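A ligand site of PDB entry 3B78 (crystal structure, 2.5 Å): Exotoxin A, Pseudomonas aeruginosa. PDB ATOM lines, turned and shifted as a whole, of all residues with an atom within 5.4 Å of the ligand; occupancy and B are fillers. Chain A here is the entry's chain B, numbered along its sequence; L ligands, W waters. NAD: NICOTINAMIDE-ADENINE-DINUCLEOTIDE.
A nitrogen (N1A) of the ligand lies close to the backbone NH of Arg 58 (2.9 Å).
The backbone carbonyl oxygen (O) of Gly 56 sits close to a nitrogen (N6A) of the ligand (3.0 Å).
The backbone carbonyl oxygen (O) of Arg 58 sits close to a nitrogen (N1A) of the ligand.
NE of Arg 60 lies close to N3A of the ligand, 3.4 Å away.
An oxygen (O7N) of the ligand sits close to the backbone NH (N) of Gly 43.
OG1 of Thr 44 lies close to O2B of the ligand, at 2.6 Å.
A nitrogen (N7N) of the ligand lies close to the backbone carbonyl oxygen (O) of Gly 43, 3.2 Å away.
The side-chain amide nitrogen (NE2) of Gln 62 lies close to an oxygen (O2A) of the ligand, at 2.7 Å.
O2D of the ligand sits close to OE2 of Glu 148 (2.9 Å).
NE2 of His 42 sits close to O2B of the ligand (3.1 Å).
The side-chain hydroxyl (OG) of Ser 51 sits close to a nitrogen (N6A) of the ligand (3.2 Å).
OE1 of Glu 155 sits close to O2D of the ligand, 3.2 Å away.
The guanidinium group of Arg 60 is in hydrogen-bond range of the backbone carbonyl oxygen of Arg 58 (3.1 Å).
O of Tyr 72 lies within hydrogen-bond range of ND1 of His 42.
OH of Tyr 83 lies within hydrogen-bond range of OE2 of Glu 148, 2.6 Å away.
The backbone NH (N) of Gly 56 lies within hydrogen-bond range of the backbone carbonyl oxygen (O) of Ser 51.
The backbone carbonyl oxygen of Tyr 83 sits close to the backbone NH of Thr 44 (3.5 Å).
The backbone NH (N) of Gly 70 sits at hydrogen-bond distance from the side-chain amide oxygen (OE1) of Gln 62 (2.6 Å).
Residues that only touch the ligand: Ala 48, Ile 52, Val 57, Phe 71, Tyr 72, Ile 73, Ala 80 and Tyr 83.
18 residues have an atom within 4 Å of the ligand: His 42, Gly 43, Thr 44, Ala 48, Ser 51, Ile 52, Gly 56, Val 57, Arg 58, Arg 60, Gln 62, Phe 71, Tyr 72, Ile 73, Ala 80, Tyr 83, Glu 148 and Glu 155.
The nearest printed residue that does not touch the ligand is Trp 160 (4.1 Å).
Water W2 lies within hydrogen-bond range of O of Gly 43 (2.6 Å) and OG1 of Thr 44 (3.3 Å).
Water W4 lies within hydrogen-bond range of O of Gly 56 and O of Ser 51.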
ATOM      1  N   TYR A  41      -8.545  30.870  -2.573  1.00  0.00           N
ATOM      2  CA  TYR A  41      -7.144  30.540  -2.340  1.00  0.00           C
ATOM      3  C   TYR A  41      -6.594  29.568  -3.385  1.00  0.00           C
ATOM      4  O   TYR A  41      -7.317  28.735  -3.928  1.00  0.00           O
ATOM      5  CB  TYR A  41      -6.956  29.913  -0.965  1.00  0.00           C
ATOM      6  CG  TYR A  41      -7.173  30.861   0.194  1.00  0.00           C
ATOM      7  CD1 TYR A  41      -6.105  31.548   0.762  1.00  0.00           C
ATOM      8  CD2 TYR A  41      -8.430  31.057   0.735  1.00  0.00           C
ATOM      9  CE1 TYR A  41      -6.295  32.407   1.823  1.00  0.00           C
ATOM     10  CE2 TYR A  41      -8.626  31.911   1.802  1.00  0.00           C
ATOM     11  CZ  TYR A  41      -7.556  32.581   2.345  1.00  0.00           C
ATOM     12  OH  TYR A  41      -7.745  33.440   3.406  1.00  0.00           O
ATOM     13  N   HIS A  42      -5.299  29.676  -3.651  1.00  0.00           N
ATOM     14  CA  HIS A  42      -4.602  28.707  -4.473  1.00  0.00           C
ATOM     15  C   HIS A  42      -3.328  28.272  -3.763  1.00  0.00           C
ATOM     16  O   HIS A  42      -2.458  29.091  -3.475  1.00  0.00           O
ATOM     17  CB  HIS A  42      -4.264  29.289  -5.849  1.00  0.00           C
ATOM     18  CG  HIS A  42      -3.497  28.360  -6.732  1.00  0.00           C
ATOM     19  ND1 HIS A  42      -4.113  27.455  -7.577  1.00  0.00           N
ATOM     20  CD2 HIS A  42      -2.166  28.189  -6.904  1.00  0.00           C
ATOM     21  CE1 HIS A  42      -3.191  26.776  -8.238  1.00  0.00           C
ATOM     22  NE2 HIS A  42      -2.001  27.196  -7.838  1.00  0.00           N
ATOM     23  N   GLY A  43      -3.226  26.983  -3.482  1.00  0.00           N
ATOM     24  CA  GLY A  43      -2.036  26.439  -2.846  1.00  0.00           C
ATOM     25  C   GLY A  43      -1.126  25.801  -3.867  1.00  0.00           C
ATOM     26  O   GLY A  43      -1.577  25.058  -4.739  1.00  0.00           O
ATOM     27  N   THR A  44       0.174  26.082  -3.767  1.00  0.00           N
ATOM     28  CA  THR A  44       1.139  25.548  -4.713  1.00  0.00           C
ATOM     29  C   THR A  44       2.559  25.551  -4.126  1.00  0.00           C
ATOM     30  O   THR A  44       2.761  25.950  -2.975  1.00  0.00           O
ATOM     31  CB  THR A  44       1.117  26.343  -6.034  1.00  0.00           C
ATOM     32  OG1 THR A  44       1.968  25.707  -7.000  1.00  0.00           O
ATOM     33  CG2 THR A  44       1.572  27.789  -5.817  1.00  0.00           C
ATOM     34  N   PHE A  45       3.534  25.089  -4.906  1.00  0.00           N
ATOM     35  CA  PHE A  45       4.917  25.069  -4.459  1.00  0.00           C
ATOM     36  C   PHE A  45       5.592  26.432  -4.631  1.00  0.00           C
ATOM     37  O   PHE A  45       5.066  27.313  -5.316  1.00  0.00           O
ATOM     38  CB  PHE A  45       5.712  23.959  -5.141  1.00  0.00           C
ATOM     39  CG  PHE A  45       5.718  24.039  -6.648  1.00  0.00           C
ATOM     40  CD1 PHE A  45       4.597  23.684  -7.379  1.00  0.00           C
ATOM     41  CD2 PHE A  45       6.856  24.456  -7.321  1.00  0.00           C
ATOM     42  CE1 PHE A  45       4.605  23.747  -8.760  1.00  0.00           C
ATOM     43  CE2 PHE A  45       6.865  24.533  -8.707  1.00  0.00           C
ATOM     44  CZ  PHE A  45       5.746  24.175  -9.424  1.00  0.00           C
ATOM     45  N   ALA A  48       6.341  28.030  -8.117  1.00  0.00           N
ATOM     46  CA  ALA A  48       5.065  28.326  -8.775  1.00  0.00           C
ATOM     47  C   ALA A  48       4.474  29.606  -8.216  1.00  0.00           C
ATOM     48  O   ALA A  48       3.907  30.416  -8.941  1.00  0.00           O
ATOM     49  CB  ALA A  48       4.100  27.170  -8.611  1.00  0.00           C
ATOM     50  N   SER A  51       6.241  32.499  -9.611  1.00  0.00           N
ATOM     51  CA  SER A  51       5.788  32.654 -10.992  1.00  0.00           C
ATOM     52  C   SER A  51       4.435  33.353 -11.061  1.00  0.00           C
ATOM     53  O   SER A  51       4.234  34.278 -11.849  1.00  0.00           O
ATOM     54  CB  SER A  51       5.703  31.288 -11.668  1.00  0.00           C
ATOM     55  OG  SER A  51       5.025  31.373 -12.906  1.00  0.00           O
ATOM     56  N   ILE A  52       3.509  32.895 -10.227  1.00  0.00           N
ATOM     57  CA  ILE A  52       2.147  33.394 -10.248  1.00  0.00           C
ATOM     58  C   ILE A  52       2.045  34.845  -9.768  1.00  0.00           C
ATOM     59  O   ILE A  52       1.330  35.653 -10.371  1.00  0.00           O
ATOM     60  CB  ILE A  52       1.230  32.499  -9.393  1.00  0.00           C
ATOM     61  CG1 ILE A  52       1.008  31.156 -10.087  1.00  0.00           C
ATOM     62  CG2 ILE A  52      -0.090  33.181  -9.114  1.00  0.00           C
ATOM     63  CD1 ILE A  52       0.238  30.148  -9.255  1.00  0.00           C
ATOM     64  N   GLY A  56       2.334  36.446 -13.164  1.00  0.00           N
ATOM     65  CA  GLY A  56       0.914  36.336 -13.432  1.00  0.00           C
ATOM     66  C   GLY A  56       0.500  34.916 -13.777  1.00  0.00           C
ATOM     67  O   GLY A  56       1.324  34.098 -14.200  1.00  0.00           O
ATOM     68  N   VAL A  57      -0.772  34.617 -13.578  1.00  0.00           N
ATOM     69  CA  VAL A  57      -1.326  33.315 -13.949  1.00  0.00           C
ATOM     70  C   VAL A  57      -1.268  33.124 -15.463  1.00  0.00           C
ATOM     71  O   VAL A  57      -1.744  33.977 -16.214  1.00  0.00           O
ATOM     72  CB  VAL A  57      -2.776  33.164 -13.445  1.00  0.00           C
ATOM     73  CG1 VAL A  57      -3.404  31.881 -13.974  1.00  0.00           C
ATOM     74  CG2 VAL A  57      -2.830  33.206 -11.925  1.00  0.00           C
ATOM     75  N   ARG A  58      -0.680  32.025 -15.914  1.00  0.00           N
ATOM     76  CA  ARG A  58      -0.552  31.736 -17.342  1.00  0.00           C
ATOM     77  C   ARG A  58      -1.067  30.341 -17.669  1.00  0.00           C
ATOM     78  O   ARG A  58      -0.761  29.375 -16.967  1.00  0.00           O
ATOM     79  CB  ARG A  58       0.905  31.855 -17.789  1.00  0.00           C
ATOM     80  CG  ARG A  58       1.624  33.101 -17.294  1.00  0.00           C
ATOM     81  CD  ARG A  58       1.469  34.262 -18.254  1.00  0.00           C
ATOM     82  NE  ARG A  58       2.372  35.352 -17.915  1.00  0.00           N
ATOM     83  CZ  ARG A  58       3.695  35.284 -18.052  1.00  0.00           C
ATOM     84  NH1 ARG A  58       4.456  36.312 -17.717  1.00  0.00           N
ATOM     85  NH2 ARG A  58       4.264  34.178 -18.511  1.00  0.00           N
ATOM     86  N   ALA A  59      -1.823  30.237 -18.760  1.00  0.00           N
ATOM     87  CA  ALA A  59      -2.367  28.952 -19.186  1.00  0.00           C
ATOM     88  C   ALA A  59      -1.258  27.922 -19.443  1.00  0.00           C
ATOM     89  O   ALA A  59      -0.185  28.262 -19.926  1.00  0.00           O
ATOM     90  CB  ALA A  59      -3.222  29.119 -20.434  1.00  0.00           C
ATOM     91  N   ARG A  60      -1.537  26.672 -19.097  1.00  0.00           N
ATOM     92  CA  ARG A  60      -0.578  25.597 -19.247  1.00  0.00           C
ATOM     93  C   ARG A  60      -1.285  24.259 -19.357  1.00  0.00           C
ATOM     94  O   ARG A  60      -2.444  24.123 -18.959  1.00  0.00           O
ATOM     95  CB  ARG A  60       0.380  25.576 -18.048  1.00  0.00           C
ATOM     96  CG  ARG A  60      -0.330  25.440 -16.707  1.00  0.00           C
ATOM     97  CD  ARG A  60       0.548  25.920 -15.564  1.00  0.00           C
ATOM     98  NE  ARG A  60       1.180  27.206 -15.857  1.00  0.00           N
ATOM     99  CZ  ARG A  60       2.487  27.372 -15.997  1.00  0.00           C
ATOM    100  NH1 ARG A  60       3.312  26.345 -15.856  1.00  0.00           N
ATOM    101  NH2 ARG A  60       2.976  28.580 -16.276  1.00  0.00           N
ATOM    102  N   GLN A  62      -2.413  20.775 -18.301  1.00  0.00           N
ATOM    103  CA  GLN A  62      -2.630  20.108 -17.028  1.00  0.00           C
ATOM    104  C   GLN A  62      -3.228  18.723 -17.240  1.00  0.00           C
ATOM    105  O   GLN A  62      -3.864  18.459 -18.261  1.00  0.00           O
ATOM    106  CB  GLN A  62      -3.509  20.973 -16.123  1.00  0.00           C
ATOM    107  CG  GLN A  62      -4.432  21.908 -16.898  1.00  0.00           C
ATOM    108  CD  GLN A  62      -5.309  22.738 -15.986  1.00  0.00           C
ATOM    109  OE1 GLN A  62      -6.341  23.235 -16.408  1.00  0.00           O
ATOM    110  NE2 GLN A  62      -4.890  22.894 -14.736  1.00  0.00           N
ATOM    111  N   ASP A  63      -3.028  17.845 -16.255  1.00  0.00           N
ATOM    112  CA  ASP A  63      -3.379  16.439 -16.412  1.00  0.00           C
ATOM    113  C   ASP A  63      -4.847  16.139 -16.102  1.00  0.00           C
ATOM    114  O   ASP A  63      -5.172  15.621 -15.032  1.00  0.00           O
ATOM    115  CB  ASP A  63      -2.463  15.571 -15.537  1.00  0.00           C
ATOM    116  CG  ASP A  63      -2.232  14.189 -16.126  1.00  0.00           C
ATOM    117  OD1 ASP A  63      -3.209  13.401 -16.185  1.00  0.00           O
ATOM    118  OD2 ASP A  63      -1.088  13.890 -16.522  1.00  0.00           O
ATOM    119  N   LEU A  64      -5.713  16.483 -17.041  1.00  0.00           N
ATOM    120  CA  LEU A  64      -7.144  16.190 -16.933  1.00  0.00           C
ATOM    121  C   LEU A  64      -7.798  16.226 -18.305  1.00  0.00           C
ATOM    122  O   LEU A  64      -7.118  16.342 -19.323  1.00  0.00           O
ATOM    123  CB  LEU A  64      -7.840  17.175 -15.978  1.00  0.00           C
ATOM    124  CG  LEU A  64      -7.458  18.662 -16.009  1.00  0.00           C
ATOM    125  CD1 LEU A  64      -7.515  19.240 -17.422  1.00  0.00           C
ATOM    126  CD2 LEU A  64      -8.355  19.452 -15.067  1.00  0.00           C
ATOM    127  N   GLY A  70      -8.420  24.741 -16.639  1.00  0.00           N
ATOM    128  CA  GLY A  70      -8.531  26.061 -16.062  1.00  0.00           C
ATOM    129  C   GLY A  70      -7.719  26.178 -14.791  1.00  0.00           C
ATOM    130  O   GLY A  70      -6.936  25.292 -14.453  1.00  0.00           O
ATOM    131  N   PHE A  71      -7.906  27.280 -14.087  1.00  0.00           N
ATOM    132  CA  PHE A  71      -7.171  27.549 -12.854  1.00  0.00           C
ATOM    133  C   PHE A  71      -8.052  27.219 -11.665  1.00  0.00           C
ATOM    134  O   PHE A  71      -9.175  27.719 -11.548  1.00  0.00           O
ATOM    135  CB  PHE A  71      -6.734  29.015 -12.819  1.00  0.00           C
ATOM    136  CG  PHE A  71      -5.722  29.318 -11.754  1.00  0.00           C
ATOM    137  CD1 PHE A  71      -4.468  28.742 -11.793  1.00  0.00           C
ATOM    138  CD2 PHE A  71      -6.022  30.209 -10.739  1.00  0.00           C
ATOM    139  CE1 PHE A  71      -3.530  29.027 -10.821  1.00  0.00           C
ATOM    140  CE2 PHE A  71      -5.082  30.505  -9.758  1.00  0.00           C
ATOM    141  CZ  PHE A  71      -3.836  29.914  -9.799  1.00  0.00           C
ATOM    142  N   TYR A  72      -7.544  26.354 -10.789  1.00  0.00           N
ATOM    143  CA  TYR A  72      -8.337  25.846  -9.676  1.00  0.00           C
ATOM    144  C   TYR A  72      -8.007  26.553  -8.364  1.00  0.00           C
ATOM    145  O   TYR A  72      -6.848  26.632  -7.957  1.00  0.00           O
ATOM    146  CB  TYR A  72      -8.134  24.341  -9.530  1.00  0.00           C
ATOM    147  CG  TYR A  72      -8.837  23.533 -10.596  1.00  0.00           C
ATOM    148  CD1 TYR A  72      -8.377  23.530 -11.907  1.00  0.00           C
ATOM    149  CD2 TYR A  72      -9.965  22.790 -10.291  1.00  0.00           C
ATOM    150  CE1 TYR A  72      -9.017  22.792 -12.884  1.00  0.00           C
ATOM    151  CE2 TYR A  72     -10.612  22.047 -11.262  1.00  0.00           C
ATOM    152  CZ  TYR A  72     -10.142  22.057 -12.556  1.00  0.00           C
ATOM    153  OH  TYR A  72     -10.782  21.316 -13.519  1.00  0.00           O
ATOM    154  N   ILE A  73      -9.050  27.067  -7.714  1.00  0.00           N
ATOM    155  CA  ILE A  73      -8.897  27.718  -6.417  1.00  0.00           C
ATOM    156  C   ILE A  73      -9.946  27.177  -5.449  1.00  0.00           C
ATOM    157  O   ILE A  73     -10.802  26.385  -5.825  1.00  0.00           O
ATOM    158  CB  ILE A  73      -9.032  29.241  -6.535  1.00  0.00           C
ATOM    159  CG1 ILE A  73     -10.455  29.627  -6.914  1.00  0.00           C
ATOM    160  CG2 ILE A  73      -8.033  29.787  -7.543  1.00  0.00           C
ATOM    161  CD1 ILE A  73     -10.668  31.119  -7.077  1.00  0.00           C
ATOM    162  N   ALA A  74      -9.874  27.634  -4.193  1.00  0.00           N
ATOM    163  CA  ALA A  74     -10.818  27.196  -3.181  1.00  0.00           C
ATOM    164  C   ALA A  74     -11.169  28.330  -2.237  1.00  0.00           C
ATOM    165  O   ALA A  74     -10.308  29.076  -1.798  1.00  0.00           O
ATOM    166  CB  ALA A  74     -10.247  26.018  -2.405  1.00  0.00           C
ATOM    167  N   LEU A  79      -8.714  23.675   2.035  1.00  0.00           N
ATOM    168  CA  LEU A  79      -8.689  22.856   0.825  1.00  0.00           C
ATOM    169  C   LEU A  79      -7.456  23.166  -0.019  1.00  0.00           C
ATOM    170  O   LEU A  79      -6.763  22.248  -0.462  1.00  0.00           O
ATOM    171  CB  LEU A  79      -9.949  23.074  -0.008  1.00  0.00           C
ATOM    172  CG  LEU A  79      -9.964  22.410  -1.387  1.00  0.00           C
ATOM    173  CD1 LEU A  79      -9.774  20.904  -1.269  1.00  0.00           C
ATOM    174  CD2 LEU A  79     -11.240  22.730  -2.149  1.00  0.00           C
ATOM    175  N   ALA A  80      -7.192  24.452  -0.248  1.00  0.00           N
ATOM    176  CA  ALA A  80      -6.047  24.867  -1.052  1.00  0.00           C
ATOM    177  C   ALA A  80      -4.740  24.552  -0.335  1.00  0.00           C
ATOM    178  O   ALA A  80      -3.704  24.376  -0.968  1.00  0.00           O
ATOM    179  CB  ALA A  80      -6.137  26.352  -1.353  1.00  0.00           C
ATOM    180  N   TYR A  83      -2.568  21.518  -1.234  1.00  0.00           N
ATOM    181  CA  TYR A  83      -1.821  21.571  -2.477  1.00  0.00           C
ATOM    182  C   TYR A  83      -0.607  22.496  -2.368  1.00  0.00           C
ATOM    183  O   TYR A  83       0.159  22.642  -3.320  1.00  0.00           O
ATOM    184  CB  TYR A  83      -2.725  22.025  -3.630  1.00  0.00           C
ATOM    185  CG  TYR A  83      -3.925  21.127  -3.828  1.00  0.00           C
ATOM    186  CD1 TYR A  83      -3.825  19.966  -4.575  1.00  0.00           C
ATOM    187  CD2 TYR A  83      -5.152  21.448  -3.264  1.00  0.00           C
ATOM    188  CE1 TYR A  83      -4.921  19.144  -4.764  1.00  0.00           C
ATOM    189  CE2 TYR A  83      -6.248  20.624  -3.439  1.00  0.00           C
ATOM    190  CZ  TYR A  83      -6.129  19.474  -4.192  1.00  0.00           C
ATOM    191  OH  TYR A  83      -7.223  18.662  -4.372  1.00  0.00           O
ATOM    192  N   GLU A 148     -15.619  19.486  -5.025  1.00  0.00           N
ATOM    193  CA  GLU A 148     -14.515  18.846  -5.739  1.00  0.00           C
ATOM    194  C   GLU A 148     -14.753  17.340  -5.850  1.00  0.00           C
ATOM    195  O   GLU A 148     -14.310  16.689  -6.782  1.00  0.00           O
ATOM    196  CB  GLU A 148     -13.183  19.101  -5.040  1.00  0.00           C
ATOM    197  CG  GLU A 148     -11.966  18.586  -5.793  1.00  0.00           C
ATOM    198  CD  GLU A 148     -10.742  18.432  -4.916  1.00  0.00           C
ATOM    199  OE1 GLU A 148     -10.903  18.110  -3.715  1.00  0.00           O
ATOM    200  OE2 GLU A 148      -9.614  18.622  -5.424  1.00  0.00           O
ATOM    201  N   GLU A 155     -14.808  23.756  -4.745  1.00  0.00           N
ATOM    202  CA  GLU A 155     -13.682  24.237  -5.521  1.00  0.00           C
ATOM    203  C   GLU A 155     -14.171  25.163  -6.625  1.00  0.00           C
ATOM    204  O   GLU A 155     -15.295  25.038  -7.107  1.00  0.00           O
ATOM    205  CB  GLU A 155     -12.880  23.075  -6.112  1.00  0.00           C
ATOM    206  CG  GLU A 155     -13.584  22.350  -7.242  1.00  0.00           C
ATOM    207  CD  GLU A 155     -12.684  21.329  -7.919  1.00  0.00           C
ATOM    208  OE1 GLU A 155     -11.457  21.385  -7.708  1.00  0.00           O
ATOM    209  OE2 GLU A 155     -13.204  20.477  -8.672  1.00  0.00           O
ATOM    210  N   TRP A 160      -9.414  29.779 -18.245  1.00  0.00           N
ATOM    211  CA  TRP A 160      -8.083  30.322 -18.464  1.00  0.00           C
ATOM    212  C   TRP A 160      -8.070  31.800 -18.858  1.00  0.00           C
ATOM    213  O   TRP A 160      -7.269  32.578 -18.344  1.00  0.00           O
ATOM    214  CB  TRP A 160      -7.285  29.482 -19.468  1.00  0.00           C
ATOM    215  CG  TRP A 160      -6.613  28.307 -18.827  1.00  0.00           C
ATOM    216  CD1 TRP A 160      -6.767  26.997 -19.150  1.00  0.00           C
ATOM    217  CD2 TRP A 160      -5.696  28.342 -17.716  1.00  0.00           C
ATOM    218  NE1 TRP A 160      -5.996  26.215 -18.329  1.00  0.00           N
ATOM    219  CE2 TRP A 160      -5.326  27.013 -17.450  1.00  0.00           C
ATOM    220  CE3 TRP A 160      -5.151  29.377 -16.949  1.00  0.00           C
ATOM    221  CZ2 TRP A 160      -4.427  26.689 -16.423  1.00  0.00           C
ATOM    222  CZ3 TRP A 160      -4.265  29.050 -15.937  1.00  0.00           C
ATOM    223  CH2 TRP A 160      -3.914  27.712 -15.679  1.00  0.00           C
HETATM  224  PA  NAD L   1      -2.516  21.811 -12.021  1.00  0.00           P
HETATM  225  O1A NAD L   1      -1.911  20.567 -12.603  1.00  0.00           O
HETATM  226  O2A NAD L   1      -3.947  22.144 -12.338  1.00  0.00           O
HETATM  227  O5B NAD L   1      -1.582  23.025 -12.518  1.00  0.00           O
HETATM  228  C5B NAD L   1      -0.167  22.766 -12.510  1.00  0.00           C
HETATM  229  C4B NAD L   1       0.600  23.778 -11.637  1.00  0.00           C
HETATM  230  O4B NAD L   1       1.192  24.861 -12.394  1.00  0.00           O
HETATM  231  C3B NAD L   1      -0.249  24.428 -10.524  1.00  0.00           C
HETATM  232  O3B NAD L   1       0.100  23.852  -9.256  1.00  0.00           O
HETATM  233  C2B NAD L   1       0.253  25.862 -10.499  1.00  0.00           C
HETATM  234  O2B NAD L   1       0.601  26.237  -9.159  1.00  0.00           O
HETATM  235  C1B NAD L   1       1.496  25.817 -11.385  1.00  0.00           C
HETATM  236  N9A NAD L   1       1.906  27.123 -11.922  1.00  0.00           N
HETATM  237  C8A NAD L   1       3.146  27.619 -11.892  1.00  0.00           C
HETATM  238  N7A NAD L   1       3.165  28.827 -12.499  1.00  0.00           N
HETATM  239  C5A NAD L   1       1.915  29.083 -12.921  1.00  0.00           C
HETATM  240  C6A NAD L   1       1.307  30.136 -13.589  1.00  0.00           C
HETATM  241  N6A NAD L   1       2.052  31.211 -13.959  1.00  0.00           N
HETATM  242  N1A NAD L   1      -0.008  30.072 -13.868  1.00  0.00           N
HETATM  243  C2A NAD L   1      -0.739  29.017 -13.503  1.00  0.00           C
HETATM  244  N3A NAD L   1      -0.189  27.984 -12.856  1.00  0.00           N
HETATM  245  C4A NAD L   1       1.131  27.991 -12.566  1.00  0.00           C
HETATM  246  O3  NAD L   1      -2.295  21.808 -10.424  1.00  0.00           O
HETATM  247  PN  NAD L   1      -3.324  22.459  -9.379  1.00  0.00           P
HETATM  248  O1N NAD L   1      -4.313  23.345 -10.096  1.00  0.00           O
HETATM  249  O2N NAD L   1      -2.552  23.000  -8.196  1.00  0.00           O
HETATM  250  O5D NAD L   1      -4.098  21.134  -8.891  1.00  0.00           O
HETATM  251  C5D NAD L   1      -5.103  20.632  -9.772  1.00  0.00           C
HETATM  252  C4D NAD L   1      -6.114  19.789  -9.010  1.00  0.00           C
HETATM  253  O4D NAD L   1      -6.157  20.134  -7.633  1.00  0.00           O
HETATM  254  C3D NAD L   1      -7.486  20.063  -9.588  1.00  0.00           C
HETATM  255  O3D NAD L   1      -7.891  18.980 -10.429  1.00  0.00           O
HETATM  256  C2D NAD L   1      -8.400  20.244  -8.390  1.00  0.00           C
HETATM  257  O2D NAD L   1      -9.294  19.128  -8.287  1.00  0.00           O
HETATM  258  C1D NAD L   1      -7.500  20.303  -7.172  1.00  0.00           C
HETATM  259  N1N NAD L   1      -7.600  21.612  -6.518  1.00  0.00           N
HETATM  260  C2N NAD L   1      -6.488  22.343  -6.348  1.00  0.00           C
HETATM  261  C3N NAD L   1      -6.529  23.585  -5.718  1.00  0.00           C
HETATM  262  C7N NAD L   1      -5.273  24.392  -5.548  1.00  0.00           C
HETATM  263  O7N NAD L   1      -5.254  25.301  -4.735  1.00  0.00           O
HETATM  264  N7N NAD L   1      -4.196  24.084  -6.268  1.00  0.00           N
HETATM  265  C4N NAD L   1      -7.748  24.069  -5.245  1.00  0.00           C
HETATM  266  C5N NAD L   1      -8.886  23.279  -5.418  1.00  0.00           C
HETATM  267  C6N NAD L   1      -8.786  22.046  -6.050  1.00  0.00           C
HETATM  268  O   HOH W   1      -2.537  25.542 -12.870  1.00  0.00           O
HETATM  269  O   HOH W   2      -0.652  23.745  -6.818  1.00  0.00           O
HETATM  270  O   HOH W   3      -4.889  25.548 -11.491  1.00  0.00           O
HETATM  271  O   HOH W   4       4.208  33.671 -14.977  1.00  0.00           O
HETATM  272  O   HOH W   5      -1.212  20.115  -8.118  1.00  0.00           O
